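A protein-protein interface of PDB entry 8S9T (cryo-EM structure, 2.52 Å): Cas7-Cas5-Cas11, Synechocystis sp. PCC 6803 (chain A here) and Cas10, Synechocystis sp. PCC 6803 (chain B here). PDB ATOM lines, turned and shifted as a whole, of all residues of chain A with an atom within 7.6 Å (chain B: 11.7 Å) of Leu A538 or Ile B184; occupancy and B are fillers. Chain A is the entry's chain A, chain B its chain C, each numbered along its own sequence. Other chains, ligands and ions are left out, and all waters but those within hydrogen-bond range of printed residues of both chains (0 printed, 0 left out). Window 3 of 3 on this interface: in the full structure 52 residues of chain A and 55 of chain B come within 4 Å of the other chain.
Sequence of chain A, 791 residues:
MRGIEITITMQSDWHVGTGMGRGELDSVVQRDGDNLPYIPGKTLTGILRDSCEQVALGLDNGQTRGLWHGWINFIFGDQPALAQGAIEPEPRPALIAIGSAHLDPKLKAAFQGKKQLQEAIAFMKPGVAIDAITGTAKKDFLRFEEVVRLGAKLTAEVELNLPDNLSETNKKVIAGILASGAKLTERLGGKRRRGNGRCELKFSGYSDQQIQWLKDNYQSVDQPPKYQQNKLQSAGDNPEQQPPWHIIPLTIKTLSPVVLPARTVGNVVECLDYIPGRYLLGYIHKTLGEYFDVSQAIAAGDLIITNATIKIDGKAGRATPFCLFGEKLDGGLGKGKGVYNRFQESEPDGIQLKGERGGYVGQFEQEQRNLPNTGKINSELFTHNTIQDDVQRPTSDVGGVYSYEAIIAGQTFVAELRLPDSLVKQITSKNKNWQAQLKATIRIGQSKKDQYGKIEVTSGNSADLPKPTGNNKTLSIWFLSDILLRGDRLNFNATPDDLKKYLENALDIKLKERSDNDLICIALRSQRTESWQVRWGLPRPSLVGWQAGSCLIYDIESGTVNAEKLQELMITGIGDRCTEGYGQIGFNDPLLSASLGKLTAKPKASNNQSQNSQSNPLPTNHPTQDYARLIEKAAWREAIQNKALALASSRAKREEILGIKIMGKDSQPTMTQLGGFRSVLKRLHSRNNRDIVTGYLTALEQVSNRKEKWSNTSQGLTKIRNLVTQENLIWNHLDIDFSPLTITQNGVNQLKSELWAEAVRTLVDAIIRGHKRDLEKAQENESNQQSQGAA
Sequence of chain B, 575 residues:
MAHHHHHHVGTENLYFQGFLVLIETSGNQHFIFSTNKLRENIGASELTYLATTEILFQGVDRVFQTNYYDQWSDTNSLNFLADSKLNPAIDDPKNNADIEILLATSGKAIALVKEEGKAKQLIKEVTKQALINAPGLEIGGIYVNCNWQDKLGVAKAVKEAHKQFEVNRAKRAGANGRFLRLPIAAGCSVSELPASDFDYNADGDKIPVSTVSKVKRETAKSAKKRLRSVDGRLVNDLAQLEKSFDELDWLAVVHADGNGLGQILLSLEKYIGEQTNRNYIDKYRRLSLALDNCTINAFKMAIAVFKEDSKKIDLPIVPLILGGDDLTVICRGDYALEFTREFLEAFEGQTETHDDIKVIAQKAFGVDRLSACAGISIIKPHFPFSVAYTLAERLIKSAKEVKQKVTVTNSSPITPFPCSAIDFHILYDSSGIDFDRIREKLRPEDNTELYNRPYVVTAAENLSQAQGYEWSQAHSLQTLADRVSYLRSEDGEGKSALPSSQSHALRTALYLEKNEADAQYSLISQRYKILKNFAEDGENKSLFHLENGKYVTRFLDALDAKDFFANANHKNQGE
OE1 of Gln A533 lies within hydrogen-bond range of N of Trp A536, at 3.0 Å.
The backbone NH of Gln A533 is in hydrogen-bond range of the backbone carbonyl oxygen of Leu A538 (3.0 Å).
The guanidinium group (NH1) of Arg B181 is in hydrogen-bond range of the backbone carbonyl oxygen (O) of Ala B185 (2.8 Å).
Of the 12 printed residues of chain A, 4 touch a printed residue of chain B.
Of the 15 printed residues of chain B, 3 touch a printed residue of chain A.
Hydrophobic or aromatic side chains of chain B that line the printed part of chain A: Pro B183 and Ile B184.
Along chain B the printed residues that touch a printed residue of chain A span positions 181 to 184.
Among the printed residues, no Asp or Glu carboxylate lies within 4 Å of a Lys or Arg side-chain nitrogen of the other chain.
CZ3 of Trp A536 touches CG of Pro B183 (3.4 Å).
CD2 of Leu A538 touches O of Pro B183 (3.6 Å).
CD1 of Leu A538 touches CD1 of Ile B184, at 3.8 Å.
Pro A539 touches Arg B181 (CG to NH1, 3.2 Å).
Pro A539 touches Pro B183 (CD to O, 3.0 Å).
CA of Pro A541 touches O of Arg B181, at 3.5 Å.
Trp A532 touches none of the printed residues of chain B.
No residue of chain B comes within 4 Å of Gln A533.
Trp A536 touches just one residue of chain B: Pro B183 (3.4 Å).
Gly A537 touches none of the printed residues of chain B.
Leu A538 touches just these residues of chain B: Pro B183 and Ile B184.
Pro A539 touches just these residues of chain B: Arg B181 (3.2 Å) and Pro B183 (3.0 Å).
Of the printed residues of chain B, Pro A541 touches Arg B181 (3.5 Å).
Printed residues of chain A within 4 Å of Arg B181: Pro A539 (3.2 Å) and Pro A541 (3.5 Å).
Ile B184 touches just one residue of chain A: Leu A538 (3.8 Å).
Ser B196 touches none of the printed residues of chain A.
The nearest residue of chain A that does not touch Ile B184 is Pro A539 (5.1 Å).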
ATOM      1  N   GLN A 229      -8.209  -8.753 -15.083  1.00  0.00           N
ATOM      2  CA  GLN A 229      -8.261  -8.567 -13.643  1.00  0.00           C
ATOM      3  C   GLN A 229      -7.033  -9.158 -12.960  1.00  0.00           C
ATOM      4  O   GLN A 229      -6.424 -10.118 -13.436  1.00  0.00           O
ATOM      5  CB  GLN A 229      -9.519  -9.195 -13.051  1.00  0.00           C
ATOM      6  CG  GLN A 229     -10.812  -8.575 -13.503  1.00  0.00           C
ATOM      7  CD  GLN A 229     -11.792  -8.403 -12.356  1.00  0.00           C
ATOM      8  OE1 GLN A 229     -11.394  -8.323 -11.195  1.00  0.00           O
ATOM      9  NE2 GLN A 229     -13.076  -8.327 -12.680  1.00  0.00           N
ATOM     10  N   SER A 531     -26.093  -4.994  -3.934  1.00  0.00           N
ATOM     11  CA  SER A 531     -24.707  -4.992  -4.437  1.00  0.00           C
ATOM     12  C   SER A 531     -24.292  -5.678  -5.750  1.00  0.00           C
ATOM     13  O   SER A 531     -25.026  -6.481  -6.322  1.00  0.00           O
ATOM     14  CB  SER A 531     -23.814  -5.604  -3.359  1.00  0.00           C
ATOM     15  OG  SER A 531     -24.006  -4.984  -2.113  1.00  0.00           O
ATOM     16  N   TRP A 532     -23.093  -5.311  -6.224  1.00  0.00           N
ATOM     17  CA  TRP A 532     -22.272  -5.930  -7.267  1.00  0.00           C
ATOM     18  C   TRP A 532     -21.227  -6.864  -6.665  1.00  0.00           C
ATOM     19  O   TRP A 532     -20.922  -6.810  -5.478  1.00  0.00           O
ATOM     20  CB  TRP A 532     -21.545  -4.885  -8.116  1.00  0.00           C
ATOM     21  CG  TRP A 532     -21.174  -5.316  -9.543  1.00  0.00           C
ATOM     22  CD1 TRP A 532     -19.922  -5.613  -9.984  1.00  0.00           C
ATOM     23  CD2 TRP A 532     -22.029  -5.452 -10.678  1.00  0.00           C
ATOM     24  NE1 TRP A 532     -19.939  -5.923 -11.301  1.00  0.00           N
ATOM     25  CE2 TRP A 532     -21.223  -5.844 -11.757  1.00  0.00           C
ATOM     26  CE3 TRP A 532     -23.393  -5.275 -10.892  1.00  0.00           C
ATOM     27  CZ2 TRP A 532     -21.729  -6.046 -13.021  1.00  0.00           C
ATOM     28  CZ3 TRP A 532     -23.891  -5.490 -12.146  1.00  0.00           C
ATOM     29  CH2 TRP A 532     -23.066  -5.875 -13.192  1.00  0.00           C
ATOM     30  N   GLN A 533     -20.610  -7.667  -7.528  1.00  0.00           N
ATOM     31  CA  GLN A 533     -19.464  -8.497  -7.178  1.00  0.00           C
ATOM     32  C   GLN A 533     -18.492  -8.165  -8.306  1.00  0.00           C
ATOM     33  O   GLN A 533     -18.626  -8.677  -9.415  1.00  0.00           O
ATOM     34  CB  GLN A 533     -19.847  -9.977  -7.138  1.00  0.00           C
ATOM     35  CG  GLN A 533     -19.266 -10.833  -6.000  1.00  0.00           C
ATOM     36  CD  GLN A 533     -17.794 -11.099  -6.073  1.00  0.00           C
ATOM     37  OE1 GLN A 533     -17.082 -10.541  -6.884  1.00  0.00           O
ATOM     38  NE2 GLN A 533     -17.322 -11.950  -5.191  1.00  0.00           N
ATOM     39  N   VAL A 534     -17.502  -7.329  -7.996  1.00  0.00           N
ATOM     40  CA  VAL A 534     -16.485  -6.877  -8.951  1.00  0.00           C
ATOM     41  C   VAL A 534     -15.637  -8.008  -9.536  1.00  0.00           C
ATOM     42  O   VAL A 534     -15.334  -8.003 -10.733  1.00  0.00           O
ATOM     43  CB  VAL A 534     -15.604  -5.813  -8.280  1.00  0.00           C
ATOM     44  CG1 VAL A 534     -14.533  -5.347  -9.213  1.00  0.00           C
ATOM     45  CG2 VAL A 534     -16.442  -4.681  -7.800  1.00  0.00           C
ATOM     46  N   ARG A 535     -15.217  -8.976  -8.727  1.00  0.00           N
ATOM     47  CA  ARG A 535     -14.519 -10.127  -9.298  1.00  0.00           C
ATOM     48  C   ARG A 535     -15.426 -10.988 -10.167  1.00  0.00           C
ATOM     49  O   ARG A 535     -14.973 -11.536 -11.176  1.00  0.00           O
ATOM     50  CB  ARG A 535     -13.888 -10.970  -8.199  1.00  0.00           C
ATOM     51  CG  ARG A 535     -13.035 -10.206  -7.251  1.00  0.00           C
ATOM     52  CD  ARG A 535     -12.378 -11.140  -6.279  1.00  0.00           C
ATOM     53  NE  ARG A 535     -11.720 -10.416  -5.207  1.00  0.00           N
ATOM     54  CZ  ARG A 535     -10.492  -9.927  -5.284  1.00  0.00           C
ATOM     55  NH1 ARG A 535      -9.772 -10.106  -6.375  1.00  0.00           N
ATOM     56  NH2 ARG A 535      -9.981  -9.271  -4.260  1.00  0.00           N
ATOM     57  N   TRP A 536     -16.692 -11.146  -9.792  1.00  0.00           N
ATOM     58  CA  TRP A 536     -17.614 -11.859 -10.664  1.00  0.00           C
ATOM     59  C   TRP A 536     -17.798 -11.143 -11.989  1.00  0.00           C
ATOM     60  O   TRP A 536     -17.968 -11.783 -13.030  1.00  0.00           O
ATOM     61  CB  TRP A 536     -18.974 -12.023  -9.999  1.00  0.00           C
ATOM     62  CG  TRP A 536     -19.048 -13.038  -8.951  1.00  0.00           C
ATOM     63  CD1 TRP A 536     -18.024 -13.710  -8.394  1.00  0.00           C
ATOM     64  CD2 TRP A 536     -20.235 -13.515  -8.319  1.00  0.00           C
ATOM     65  NE1 TRP A 536     -18.487 -14.578  -7.448  1.00  0.00           N
ATOM     66  CE2 TRP A 536     -19.847 -14.473  -7.381  1.00  0.00           C
ATOM     67  CE3 TRP A 536     -21.588 -13.206  -8.445  1.00  0.00           C
ATOM     68  CZ2 TRP A 536     -20.749 -15.130  -6.585  1.00  0.00           C
ATOM     69  CZ3 TRP A 536     -22.480 -13.869  -7.653  1.00  0.00           C
ATOM     70  CH2 TRP A 536     -22.061 -14.820  -6.738  1.00  0.00           C
ATOM     71  N   GLY A 537     -17.793  -9.819 -11.973  1.00  0.00           N
ATOM     72  CA  GLY A 537     -18.110  -9.112 -13.176  1.00  0.00           C
ATOM     73  C   GLY A 537     -19.595  -8.977 -13.347  1.00  0.00           C
ATOM     74  O   GLY A 537     -20.057  -8.480 -14.378  1.00  0.00           O
ATOM     75  N   LEU A 538     -20.345  -9.374 -12.333  1.00  0.00           N
ATOM     76  CA  LEU A 538     -21.782  -9.544 -12.403  1.00  0.00           C
ATOM     77  C   LEU A 538     -22.358  -9.142 -11.063  1.00  0.00           C
ATOM     78  O   LEU A 538     -21.619  -8.953 -10.094  1.00  0.00           O
ATOM     79  CB  LEU A 538     -22.125 -11.001 -12.708  1.00  0.00           C
ATOM     80  CG  LEU A 538     -21.999 -11.449 -14.148  1.00  0.00           C
ATOM     81  CD1 LEU A 538     -22.453 -12.869 -14.243  1.00  0.00           C
ATOM     82  CD2 LEU A 538     -22.819 -10.542 -15.022  1.00  0.00           C
ATOM     83  N   PRO A 539     -23.669  -8.961 -10.984  1.00  0.00           N
ATOM     84  CA  PRO A 539     -24.274  -8.516  -9.731  1.00  0.00           C
ATOM     85  C   PRO A 539     -24.171  -9.581  -8.669  1.00  0.00           C
ATOM     86  O   PRO A 539     -24.078 -10.772  -8.964  1.00  0.00           O
ATOM     87  CB  PRO A 539     -25.740  -8.279 -10.100  1.00  0.00           C
ATOM     88  CG  PRO A 539     -25.793  -8.214 -11.509  1.00  0.00           C
ATOM     89  CD  PRO A 539     -24.611  -8.857 -12.105  1.00  0.00           C
ATOM     90  N   ARG A 540     -24.149  -9.150  -7.431  1.00  0.00           N
ATOM     91  CA  ARG A 540     -24.239 -10.133  -6.381  1.00  0.00           C
ATOM     92  C   ARG A 540     -25.685 -10.578  -6.261  1.00  0.00           C
ATOM     93  O   ARG A 540     -26.595  -9.869  -6.683  1.00  0.00           O
ATOM     94  CB  ARG A 540     -23.834  -9.516  -5.059  1.00  0.00           C
ATOM     95  CG  ARG A 540     -22.541  -9.893  -4.441  1.00  0.00           C
ATOM     96  CD  ARG A 540     -22.310  -8.828  -3.412  1.00  0.00           C
ATOM     97  NE  ARG A 540     -21.770  -9.332  -2.170  1.00  0.00           N
ATOM     98  CZ  ARG A 540     -21.975  -8.768  -0.990  1.00  0.00           C
ATOM     99  NH1 ARG A 540     -22.745  -7.704  -0.874  1.00  0.00           N
ATOM    100  NH2 ARG A 540     -21.430  -9.301   0.077  1.00  0.00           N
ATOM    101  N   PRO A 541     -25.929 -11.767  -5.732  1.00  0.00           N
ATOM    102  CA  PRO A 541     -27.306 -12.173  -5.480  1.00  0.00           C
ATOM    103  C   PRO A 541     -27.921 -11.248  -4.447  1.00  0.00           C
ATOM    104  O   PRO A 541     -27.240 -10.745  -3.556  1.00  0.00           O
ATOM    105  CB  PRO A 541     -27.158 -13.599  -4.956  1.00  0.00           C
ATOM    106  CG  PRO A 541     -25.770 -13.661  -4.496  1.00  0.00           C
ATOM    107  CD  PRO A 541     -25.019 -12.888  -5.487  1.00  0.00           C
ATOM    108  N   LEU B 180     -36.023 -11.414  -6.758  1.00  0.00           N
ATOM    109  CA  LEU B 180     -34.637 -11.283  -6.334  1.00  0.00           C
ATOM    110  C   LEU B 180     -33.655 -11.384  -7.488  1.00  0.00           C
ATOM    111  O   LEU B 180     -33.784 -12.239  -8.368  1.00  0.00           O
ATOM    112  CB  LEU B 180     -34.276 -12.332  -5.284  1.00  0.00           C
ATOM    113  CG  LEU B 180     -34.987 -12.282  -3.937  1.00  0.00           C
ATOM    114  CD1 LEU B 180     -34.633 -13.482  -3.105  1.00  0.00           C
ATOM    115  CD2 LEU B 180     -34.569 -11.030  -3.221  1.00  0.00           C
ATOM    116  N   ARG B 181     -32.661 -10.500  -7.447  1.00  0.00           N
ATOM    117  CA  ARG B 181     -31.565 -10.492  -8.403  1.00  0.00           C
ATOM    118  C   ARG B 181     -30.723 -11.755  -8.403  1.00  0.00           C
ATOM    119  O   ARG B 181     -30.275 -12.238  -7.362  1.00  0.00           O
ATOM    120  CB  ARG B 181     -30.653  -9.281  -8.242  1.00  0.00           C
ATOM    121  CG  ARG B 181     -29.827  -9.097  -9.523  1.00  0.00           C
ATOM    122  CD  ARG B 181     -30.505  -8.379 -10.672  1.00  0.00           C
ATOM    123  NE  ARG B 181     -30.272  -6.948 -10.679  1.00  0.00           N
ATOM    124  CZ  ARG B 181     -29.377  -6.358 -11.458  1.00  0.00           C
ATOM    125  NH1 ARG B 181     -28.670  -7.074 -12.307  1.00  0.00           N
ATOM    126  NH2 ARG B 181     -29.200  -5.050 -11.405  1.00  0.00           N
ATOM    127  N   LEU B 182     -30.500 -12.262  -9.607  1.00  0.00           N
ATOM    128  CA  LEU B 182     -29.711 -13.415  -9.904  1.00  0.00           C
ATOM    129  C   LEU B 182     -28.564 -12.808 -10.689  1.00  0.00           C
ATOM    130  O   LEU B 182     -28.809 -11.941 -11.535  1.00  0.00           O
ATOM    131  CB  LEU B 182     -30.479 -14.414 -10.772  1.00  0.00           C
ATOM    132  CG  LEU B 182     -30.933 -15.760 -10.220  1.00  0.00           C
ATOM    133  CD1 LEU B 182     -29.830 -16.434  -9.449  1.00  0.00           C
ATOM    134  CD2 LEU B 182     -32.149 -15.586  -9.358  1.00  0.00           C
ATOM    135  N   PRO B 183     -27.315 -13.160 -10.395  1.00  0.00           N
ATOM    136  CA  PRO B 183     -26.182 -12.507 -11.079  1.00  0.00           C
ATOM    137  C   PRO B 183     -26.291 -12.371 -12.589  1.00  0.00           C
ATOM    138  O   PRO B 183     -25.702 -11.450 -13.156  1.00  0.00           O
ATOM    139  CB  PRO B 183     -25.015 -13.406 -10.681  1.00  0.00           C
ATOM    140  CG  PRO B 183     -25.398 -13.901  -9.354  1.00  0.00           C
ATOM    141  CD  PRO B 183     -26.864 -14.102  -9.364  1.00  0.00           C
ATOM    142  N   ILE B 184     -27.039 -13.242 -13.260  1.00  0.00           N
ATOM    143  CA  ILE B 184     -27.132 -13.210 -14.714  1.00  0.00           C
ATOM    144  C   ILE B 184     -28.352 -12.449 -15.219  1.00  0.00           C
ATOM    145  O   ILE B 184     -28.399 -12.093 -16.405  1.00  0.00           O
ATOM    146  CB  ILE B 184     -27.038 -14.658 -15.244  1.00  0.00           C
ATOM    147  CG1 ILE B 184     -25.575 -15.056 -15.293  1.00  0.00           C
ATOM    148  CG2 ILE B 184     -27.608 -14.844 -16.615  1.00  0.00           C
ATOM    149  CD1 ILE B 184     -25.075 -15.645 -14.059  1.00  0.00           C
ATOM    150  N   ALA B 185     -29.278 -12.087 -14.344  1.00  0.00           N
ATOM    151  CA  ALA B 185     -30.365 -11.199 -14.725  1.00  0.00           C
ATOM    152  C   ALA B 185     -29.899  -9.757 -14.877  1.00  0.00           C
ATOM    153  O   ALA B 185     -29.121  -9.249 -14.075  1.00  0.00           O
ATOM    154  CB  ALA B 185     -31.495 -11.271 -13.702  1.00  0.00           C
ATOM    155  N   ALA B 186     -30.390  -9.105 -15.922  1.00  0.00           N
ATOM    156  CA  ALA B 186     -30.117  -7.710 -16.185  1.00  0.00           C
ATOM    157  C   ALA B 186     -30.941  -6.863 -15.225  1.00  0.00           C
ATOM    158  O   ALA B 186     -31.895  -7.338 -14.607  1.00  0.00           O
ATOM    159  CB  ALA B 186     -30.444  -7.366 -17.631  1.00  0.00           C
ATOM    160  N   GLY B 187     -30.611  -5.591 -15.117  1.00  0.00           N
ATOM    161  CA  GLY B 187     -31.431  -4.812 -14.225  1.00  0.00           C
ATOM    162  C   GLY B 187     -32.432  -3.874 -14.854  1.00  0.00           C
ATOM    163  O   GLY B 187     -32.340  -3.521 -16.026  1.00  0.00           O
ATOM    164  N   CYS B 188     -33.427  -3.503 -14.061  1.00  0.00           N
ATOM    165  CA  CYS B 188     -34.416  -2.527 -14.475  1.00  0.00           C
ATOM    166  C   CYS B 188     -33.740  -1.210 -14.815  1.00  0.00           C
ATOM    167  O   CYS B 188     -32.733  -0.835 -14.218  1.00  0.00           O
ATOM    168  CB  CYS B 188     -35.452  -2.334 -13.376  1.00  0.00           C
ATOM    169  SG  CYS B 188     -36.777  -1.210 -13.772  1.00  0.00           S
ATOM    170  N   LEU B 193     -34.617  -3.481  -8.975  1.00  0.00           N
ATOM    171  CA  LEU B 193     -34.999  -4.860  -9.216  1.00  0.00           C
ATOM    172  C   LEU B 193     -34.382  -5.391 -10.500  1.00  0.00           C
ATOM    173  O   LEU B 193     -33.946  -4.620 -11.358  1.00  0.00           O
ATOM    174  CB  LEU B 193     -36.515  -4.973  -9.275  1.00  0.00           C
ATOM    175  CG  LEU B 193     -37.292  -4.634  -8.007  1.00  0.00           C
ATOM    176  CD1 LEU B 193     -38.736  -4.898  -8.259  1.00  0.00           C
ATOM    177  CD2 LEU B 193     -36.827  -5.427  -6.833  1.00  0.00           C
ATOM    178  N   PRO B 194     -34.296  -6.712 -10.652  1.00  0.00           N
ATOM    179  CA  PRO B 194     -33.959  -7.271 -11.962  1.00  0.00           C
ATOM    180  C   PRO B 194     -34.997  -6.912 -13.017  1.00  0.00           C
ATOM    181  O   PRO B 194     -36.194  -6.823 -12.746  1.00  0.00           O
ATOM    182  CB  PRO B 194     -33.927  -8.776 -11.696  1.00  0.00           C
ATOM    183  CG  PRO B 194     -34.824  -8.968 -10.565  1.00  0.00           C
ATOM    184  CD  PRO B 194     -34.633  -7.772  -9.692  1.00  0.00           C
ATOM    185  N   ALA B 195     -34.520  -6.743 -14.244  1.00  0.00           N
ATOM    186  CA  ALA B 195     -35.412  -6.548 -15.371  1.00  0.00           C
ATOM    187  C   ALA B 195     -36.157  -7.832 -15.680  1.00  0.00           C
ATOM    188  O   ALA B 195     -35.662  -8.937 -15.456  1.00  0.00           O
ATOM    189  CB  ALA B 195     -34.637  -6.071 -16.594  1.00  0.00           C
ATOM    190  N   SER B 196     -37.378  -7.673 -16.168  1.00  0.00           N
ATOM    191  CA  SER B 196     -38.265  -8.803 -16.372  1.00  0.00           C
ATOM    192  C   SER B 196     -38.847  -8.760 -17.773  1.00  0.00           C
ATOM    193  O   SER B 196     -39.111  -9.802 -18.374  1.00  0.00           O
ATOM    194  CB  SER B 196     -39.355  -8.804 -15.313  1.00  0.00           C
ATOM    195  OG  SER B 196     -40.355  -9.755 -15.601  1.00  0.00           O
ATOM    196  N   PHE B 198     -39.714  -5.471 -21.149  1.00  0.00           N
ATOM    197  CA  PHE B 198     -39.322  -4.230 -21.793  1.00  0.00           C
ATOM    198  C   PHE B 198     -40.463  -3.230 -21.797  1.00  0.00           C
ATOM    199  O   PHE B 198     -41.634  -3.595 -21.865  1.00  0.00           O
ATOM    200  CB  PHE B 198     -38.850  -4.475 -23.223  1.00  0.00           C
ATOM    201  CG  PHE B 198     -37.540  -5.173 -23.299  1.00  0.00           C
ATOM    202  CD1 PHE B 198     -36.368  -4.455 -23.265  1.00  0.00           C
ATOM    203  CD2 PHE B 198     -37.480  -6.542 -23.399  1.00  0.00           C
ATOM    204  CE1 PHE B 198     -35.169  -5.091 -23.318  1.00  0.00           C
ATOM    205  CE2 PHE B 198     -36.287  -7.177 -23.464  1.00  0.00           C
ATOM    206  CZ  PHE B 198     -35.131  -6.456 -23.421  1.00  0.00           C
ATOM    207  N   PRO B 208     -35.226  -2.138 -20.660  1.00  0.00           N
ATOM    208  CA  PRO B 208     -35.625  -3.213 -19.747  1.00  0.00           C
ATOM    209  C   PRO B 208     -36.193  -2.677 -18.439  1.00  0.00           C
ATOM    210  O   PRO B 208     -35.648  -1.756 -17.832  1.00  0.00           O
ATOM    211  CB  PRO B 208     -34.316  -3.972 -19.528  1.00  0.00           C
ATOM    212  CG  PRO B 208     -33.285  -2.946 -19.693  1.00  0.00           C
ATOM    213  CD  PRO B 208     -33.764  -2.020 -20.757  1.00  0.00           C
